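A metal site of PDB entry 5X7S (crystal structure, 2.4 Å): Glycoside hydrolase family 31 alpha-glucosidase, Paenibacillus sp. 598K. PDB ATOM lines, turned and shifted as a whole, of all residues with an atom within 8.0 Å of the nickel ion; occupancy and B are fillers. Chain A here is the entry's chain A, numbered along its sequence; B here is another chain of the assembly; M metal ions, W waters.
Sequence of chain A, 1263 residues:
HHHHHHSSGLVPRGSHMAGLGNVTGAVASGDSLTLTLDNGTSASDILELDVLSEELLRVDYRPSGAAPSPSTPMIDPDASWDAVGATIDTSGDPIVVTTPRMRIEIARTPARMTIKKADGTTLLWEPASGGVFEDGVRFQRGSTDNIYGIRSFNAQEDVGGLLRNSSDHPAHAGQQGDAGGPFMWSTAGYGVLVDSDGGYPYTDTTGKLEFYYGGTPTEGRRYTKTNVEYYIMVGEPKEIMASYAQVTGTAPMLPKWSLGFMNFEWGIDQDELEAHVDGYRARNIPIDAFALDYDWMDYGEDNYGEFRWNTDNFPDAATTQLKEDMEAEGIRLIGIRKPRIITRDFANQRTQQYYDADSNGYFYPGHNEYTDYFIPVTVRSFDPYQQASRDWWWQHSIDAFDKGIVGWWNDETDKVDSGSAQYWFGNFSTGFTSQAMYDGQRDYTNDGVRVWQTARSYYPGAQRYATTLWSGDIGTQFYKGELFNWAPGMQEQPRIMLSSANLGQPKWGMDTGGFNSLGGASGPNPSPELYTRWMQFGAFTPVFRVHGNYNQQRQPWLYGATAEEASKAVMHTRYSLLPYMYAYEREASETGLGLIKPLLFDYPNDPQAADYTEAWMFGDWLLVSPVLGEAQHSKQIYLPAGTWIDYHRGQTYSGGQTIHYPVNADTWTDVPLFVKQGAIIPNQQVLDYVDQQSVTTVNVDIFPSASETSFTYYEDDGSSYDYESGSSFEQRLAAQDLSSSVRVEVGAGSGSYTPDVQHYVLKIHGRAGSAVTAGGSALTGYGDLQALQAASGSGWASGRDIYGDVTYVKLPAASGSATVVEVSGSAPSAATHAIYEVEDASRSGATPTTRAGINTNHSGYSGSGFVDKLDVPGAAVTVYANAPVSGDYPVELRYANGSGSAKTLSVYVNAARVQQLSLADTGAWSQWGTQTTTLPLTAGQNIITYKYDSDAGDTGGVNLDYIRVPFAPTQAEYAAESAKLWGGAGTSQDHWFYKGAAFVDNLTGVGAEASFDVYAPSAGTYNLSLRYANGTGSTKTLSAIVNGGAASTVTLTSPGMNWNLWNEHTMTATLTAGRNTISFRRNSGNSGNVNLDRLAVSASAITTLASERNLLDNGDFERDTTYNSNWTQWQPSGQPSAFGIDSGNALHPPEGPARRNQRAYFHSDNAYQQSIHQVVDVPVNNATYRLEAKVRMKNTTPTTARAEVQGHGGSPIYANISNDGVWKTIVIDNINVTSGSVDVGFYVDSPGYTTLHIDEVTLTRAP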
ATOM      1  N   ILE A 150      -9.071 -11.219  25.714  1.00  0.00           N
ATOM      2  CA  ILE A 150      -8.684 -10.239  26.732  1.00  0.00           C
ATOM      3  C   ILE A 150      -8.819  -8.775  26.317  1.00  0.00           C
ATOM      4  O   ILE A 150      -9.297  -7.935  27.108  1.00  0.00           O
ATOM      5  CB  ILE A 150      -7.255 -10.471  27.223  1.00  0.00           C
ATOM      6  CG1 ILE A 150      -7.127 -11.853  27.866  1.00  0.00           C
ATOM      7  CG2 ILE A 150      -6.829  -9.377  28.213  1.00  0.00           C
ATOM      8  CD1 ILE A 150      -5.687 -12.338  27.918  1.00  0.00           C
ATOM      9  N   ARG A 151      -8.295  -8.438  25.136  1.00  0.00           N
ATOM     10  CA  ARG A 151      -8.094  -7.040  24.781  1.00  0.00           C
ATOM     11  C   ARG A 151      -7.830  -6.877  23.305  1.00  0.00           C
ATOM     12  O   ARG A 151      -7.464  -7.856  22.591  1.00  0.00           O
ATOM     13  CB  ARG A 151      -6.904  -6.405  25.545  1.00  0.00           C
ATOM     14  CG  ARG A 151      -5.529  -7.047  25.368  1.00  0.00           C
ATOM     15  CD  ARG A 151      -4.739  -6.498  24.210  1.00  0.00           C
ATOM     16  NE  ARG A 151      -4.334  -5.137  24.510  1.00  0.00           N
ATOM     17  CZ  ARG A 151      -3.150  -4.769  25.000  1.00  0.00           C
ATOM     18  NH1 ARG A 151      -2.222  -5.668  25.301  1.00  0.00           N
ATOM     19  NH2 ARG A 151      -2.898  -3.487  25.229  1.00  0.00           N
ATOM     20  N   SER A 152      -7.987  -5.604  22.914  1.00  0.00           N
ATOM     21  CA  SER A 152      -7.623  -5.068  21.611  1.00  0.00           C
ATOM     22  C   SER A 152      -6.748  -3.799  21.844  1.00  0.00           C
ATOM     23  O   SER A 152      -6.107  -3.663  22.887  1.00  0.00           O
ATOM     24  CB  SER A 152      -8.907  -4.749  20.854  1.00  0.00           C
ATOM     25  OG  SER A 152      -8.593  -4.171  19.611  1.00  0.00           O
ATOM     26  N   PHE A 153      -6.704  -2.863  20.892  1.00  0.00           N
ATOM     27  CA  PHE A 153      -5.839  -1.673  21.009  1.00  0.00           C
ATOM     28  C   PHE A 153      -6.553  -0.420  20.573  1.00  0.00           C
ATOM     29  O   PHE A 153      -7.398  -0.474  19.679  1.00  0.00           O
ATOM     30  CB  PHE A 153      -4.599  -1.846  20.191  1.00  0.00           C
ATOM     31  CG  PHE A 153      -3.927  -3.111  20.423  1.00  0.00           C
ATOM     32  CD1 PHE A 153      -2.965  -3.219  21.451  1.00  0.00           C
ATOM     33  CD2 PHE A 153      -4.242  -4.206  19.657  1.00  0.00           C
ATOM     34  CE1 PHE A 153      -2.328  -4.415  21.693  1.00  0.00           C
ATOM     35  CE2 PHE A 153      -3.600  -5.408  19.905  1.00  0.00           C
ATOM     36  CZ  PHE A 153      -2.639  -5.505  20.910  1.00  0.00           C
ATOM     37  N   ASN A 154      -6.246   0.692  21.237  1.00  0.00           N
ATOM     38  CA  ASN A 154      -7.016   1.932  21.017  1.00  0.00           C
ATOM     39  C   ASN A 154      -6.324   2.870  19.993  1.00  0.00           C
ATOM     40  O   ASN A 154      -5.273   2.570  19.500  1.00  0.00           O
ATOM     41  CB  ASN A 154      -7.404   2.589  22.365  1.00  0.00           C
ATOM     42  CG  ASN A 154      -6.245   3.257  23.106  1.00  0.00           C
ATOM     43  OD1 ASN A 154      -5.179   3.469  22.554  1.00  0.00           O
ATOM     44  ND2 ASN A 154      -6.469   3.587  24.384  1.00  0.00           N
ATOM     45  N   GLU A 157      -2.439   3.958  21.141  1.00  0.00           N
ATOM     46  CA  GLU A 157      -1.653   2.864  21.730  1.00  0.00           C
ATOM     47  C   GLU A 157      -0.795   2.258  20.635  1.00  0.00           C
ATOM     48  O   GLU A 157      -1.218   2.223  19.489  1.00  0.00           O
ATOM     49  CB  GLU A 157      -2.561   1.757  22.299  1.00  0.00           C
ATOM     50  CG  GLU A 157      -2.863   1.859  23.786  1.00  0.00           C
ATOM     51  CD  GLU A 157      -3.612   0.652  24.350  1.00  0.00           C
ATOM     52  OE1 GLU A 157      -4.482   0.052  23.644  1.00  0.00           O
ATOM     53  OE2 GLU A 157      -3.323   0.281  25.515  1.00  0.00           O
ATOM     54  N   HIS A 169      -2.445  -7.205  30.686  1.00  0.00           N
ATOM     55  CA  HIS A 169      -3.325  -6.041  30.455  1.00  0.00           C
ATOM     56  C   HIS A 169      -4.664  -6.265  31.144  1.00  0.00           C
ATOM     57  O   HIS A 169      -5.165  -7.353  31.119  1.00  0.00           O
ATOM     58  CB  HIS A 169      -3.579  -5.848  28.969  1.00  0.00           C
ATOM     59  CG  HIS A 169      -4.087  -4.484  28.600  1.00  0.00           C
ATOM     60  ND1 HIS A 169      -3.277  -3.366  28.612  1.00  0.00           N
ATOM     61  CD2 HIS A 169      -5.299  -4.072  28.187  1.00  0.00           C
ATOM     62  CE1 HIS A 169      -3.978  -2.321  28.185  1.00  0.00           C
ATOM     63  NE2 HIS A 169      -5.209  -2.735  27.936  1.00  0.00           N
ATOM     64  N   PRO A 170      -5.255  -5.230  31.749  1.00  0.00           N
ATOM     65  CA  PRO A 170      -6.571  -5.435  32.332  1.00  0.00           C
ATOM     66  C   PRO A 170      -7.628  -5.762  31.308  1.00  0.00           C
ATOM     67  O   PRO A 170      -7.458  -5.465  30.126  1.00  0.00           O
ATOM     68  CB  PRO A 170      -6.910  -4.097  33.018  1.00  0.00           C
ATOM     69  CG  PRO A 170      -5.660  -3.288  33.033  1.00  0.00           C
ATOM     70  CD  PRO A 170      -4.686  -3.905  32.068  1.00  0.00           C
ATOM     71  N   ALA A 171      -8.718  -6.366  31.786  1.00  0.00           N
ATOM     72  CA  ALA A 171      -9.877  -6.590  31.003  1.00  0.00           C
ATOM     73  C   ALA A 171     -10.735  -5.333  31.232  1.00  0.00           C
ATOM     74  O   ALA A 171     -11.098  -5.033  32.363  1.00  0.00           O
ATOM     75  CB  ALA A 171     -10.568  -7.841  31.459  1.00  0.00           C
ATOM     76  N   HIS A 172     -10.993  -4.576  30.182  1.00  0.00           N
ATOM     77  CA  HIS A 172     -11.867  -3.392  30.253  1.00  0.00           C
ATOM     78  C   HIS A 172     -12.431  -3.038  28.886  1.00  0.00           C
ATOM     79  O   HIS A 172     -11.889  -3.442  27.839  1.00  0.00           O
ATOM     80  CB  HIS A 172     -11.157  -2.184  30.822  1.00  0.00           C
ATOM     81  CG  HIS A 172      -9.860  -1.839  30.142  1.00  0.00           C
ATOM     82  ND1 HIS A 172      -8.680  -1.721  30.841  1.00  0.00           N
ATOM     83  CD2 HIS A 172      -9.556  -1.586  28.847  1.00  0.00           C
ATOM     84  CE1 HIS A 172      -7.693  -1.435  30.007  1.00  0.00           C
ATOM     85  NE2 HIS A 172      -8.205  -1.332  28.783  1.00  0.00           N
ATOM     86  N   ALA A 173     -13.504  -2.267  28.909  1.00  0.00           N
ATOM     87  CA  ALA A 173     -14.071  -1.672  27.696  1.00  0.00           C
ATOM     88  C   ALA A 173     -13.058  -0.731  27.060  1.00  0.00           C
ATOM     89  O   ALA A 173     -12.764  -0.850  25.892  1.00  0.00           O
ATOM     90  CB  ALA A 173     -15.373  -0.921  28.013  1.00  0.00           C
ATOM     91  N   GLY A 174     -12.509   0.188  27.863  1.00  0.00           N
ATOM     92  CA  GLY A 174     -11.437   1.112  27.415  1.00  0.00           C
ATOM     93  C   GLY A 174     -11.951   2.372  26.785  1.00  0.00           C
ATOM     94  O   GLY A 174     -13.053   2.831  27.105  1.00  0.00           O
ATOM     95  N   GLN A 175     -11.147   2.951  25.897  1.00  0.00           N
ATOM     96  CA  GLN A 175     -11.569   4.138  25.128  1.00  0.00           C
ATOM     97  C   GLN A 175     -11.098   4.103  23.682  1.00  0.00           C
ATOM     98  O   GLN A 175     -10.187   3.356  23.344  1.00  0.00           O
ATOM     99  CB  GLN A 175     -11.017   5.400  25.789  1.00  0.00           C
ATOM    100  CG  GLN A 175      -9.483   5.448  25.839  1.00  0.00           C
ATOM    101  CD  GLN A 175      -8.902   6.758  26.372  1.00  0.00           C
ATOM    102  OE1 GLN A 175      -9.340   7.873  26.004  1.00  0.00           O
ATOM    103  NE2 GLN A 175      -7.915   6.625  27.252  1.00  0.00           N
ATOM    104  N   ASP A 178     -10.931   0.811  21.713  1.00  0.00           N
ATOM    105  CA  ASP A 178     -10.573  -0.388  22.444  1.00  0.00           C
ATOM    106  C   ASP A 178     -11.728  -1.334  22.595  1.00  0.00           C
ATOM    107  O   ASP A 178     -12.905  -0.971  22.460  1.00  0.00           O
ATOM    108  CB  ASP A 178     -10.032  -0.055  23.833  1.00  0.00           C
ATOM    109  CG  ASP A 178      -8.889  -0.987  24.301  1.00  0.00           C
ATOM    110  OD1 ASP A 178      -8.677  -2.136  23.805  1.00  0.00           O
ATOM    111  OD2 ASP A 178      -8.208  -0.529  25.218  1.00  0.00           O
ATOM    112  N   ALA A 179     -11.347  -2.553  22.946  1.00  0.00           N
ATOM    113  CA  ALA A 179     -12.287  -3.569  23.383  1.00  0.00           C
ATOM    114  C   ALA A 179     -11.563  -4.514  24.315  1.00  0.00           C
ATOM    115  O   ALA A 179     -10.339  -4.606  24.325  1.00  0.00           O
ATOM    116  CB  ALA A 179     -12.814  -4.316  22.177  1.00  0.00           C
ATOM    117  N   GLY A 180     -12.324  -5.228  25.117  1.00  0.00           N
ATOM    118  CA  GLY A 180     -11.733  -6.140  26.055  1.00  0.00           C
ATOM    119  C   GLY A 180     -12.771  -6.800  26.955  1.00  0.00           C
ATOM    120  O   GLY A 180     -14.000  -6.472  26.927  1.00  0.00           O
ATOM    121  N   TRP B 424     -13.655   8.510  33.900  1.00  0.00           N
ATOM    122  CA  TRP B 424     -13.927   7.284  33.184  1.00  0.00           C
ATOM    123  C   TRP B 424     -15.401   6.940  33.249  1.00  0.00           C
ATOM    124  O   TRP B 424     -16.016   7.177  34.264  1.00  0.00           O
ATOM    125  CB  TRP B 424     -13.120   6.153  33.761  1.00  0.00           C
ATOM    126  CG  TRP B 424     -11.688   6.109  33.252  1.00  0.00           C
ATOM    127  CD1 TRP B 424     -10.595   6.646  33.856  1.00  0.00           C
ATOM    128  CD2 TRP B 424     -11.218   5.463  32.056  1.00  0.00           C
ATOM    129  NE1 TRP B 424      -9.470   6.395  33.105  1.00  0.00           N
ATOM    130  CE2 TRP B 424      -9.819   5.660  32.008  1.00  0.00           C
ATOM    131  CE3 TRP B 424     -11.851   4.741  31.027  1.00  0.00           C
ATOM    132  CZ2 TRP B 424      -9.027   5.166  30.969  1.00  0.00           C
ATOM    133  CZ3 TRP B 424     -11.064   4.254  29.982  1.00  0.00           C
ATOM    134  CH2 TRP B 424      -9.668   4.459  29.966  1.00  0.00           C
HETATM  135 NI    NI M   1      -6.912  -1.655  26.809  1.00  0.00          NI
HETATM  136  O   HOH W   1      -8.111  -3.513  26.100  1.00  0.00           O
HETATM  137  O   HOH W   2      -6.139   0.167  26.689  1.00  0.00           O
HETATM  138  O   HOH W   3      -5.728  -1.916  25.008  1.00  0.00           O
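A ring nitrogen (ND1) of His 169 lies close to the guanidinium group (NH2) of Arg 151. O of His 172 sits close to N of Gly 180 (3.3 Å).
The nickel ion is bound by water W2 (2.0 Å), water W3 (2.2 Å), NE2 of His 169 (2.3 Å), water W1 (2.3 Å), OD2 of Asp 178 (2.3 Å) and NE2 of His 172 (2.4 Å). The nickel ion has six donor atoms within binding distance.
Water W1 lies within hydrogen-bond range of OD1 of Asp 178 (2.7 Å) and O of Ala 179 (3.1 Å).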
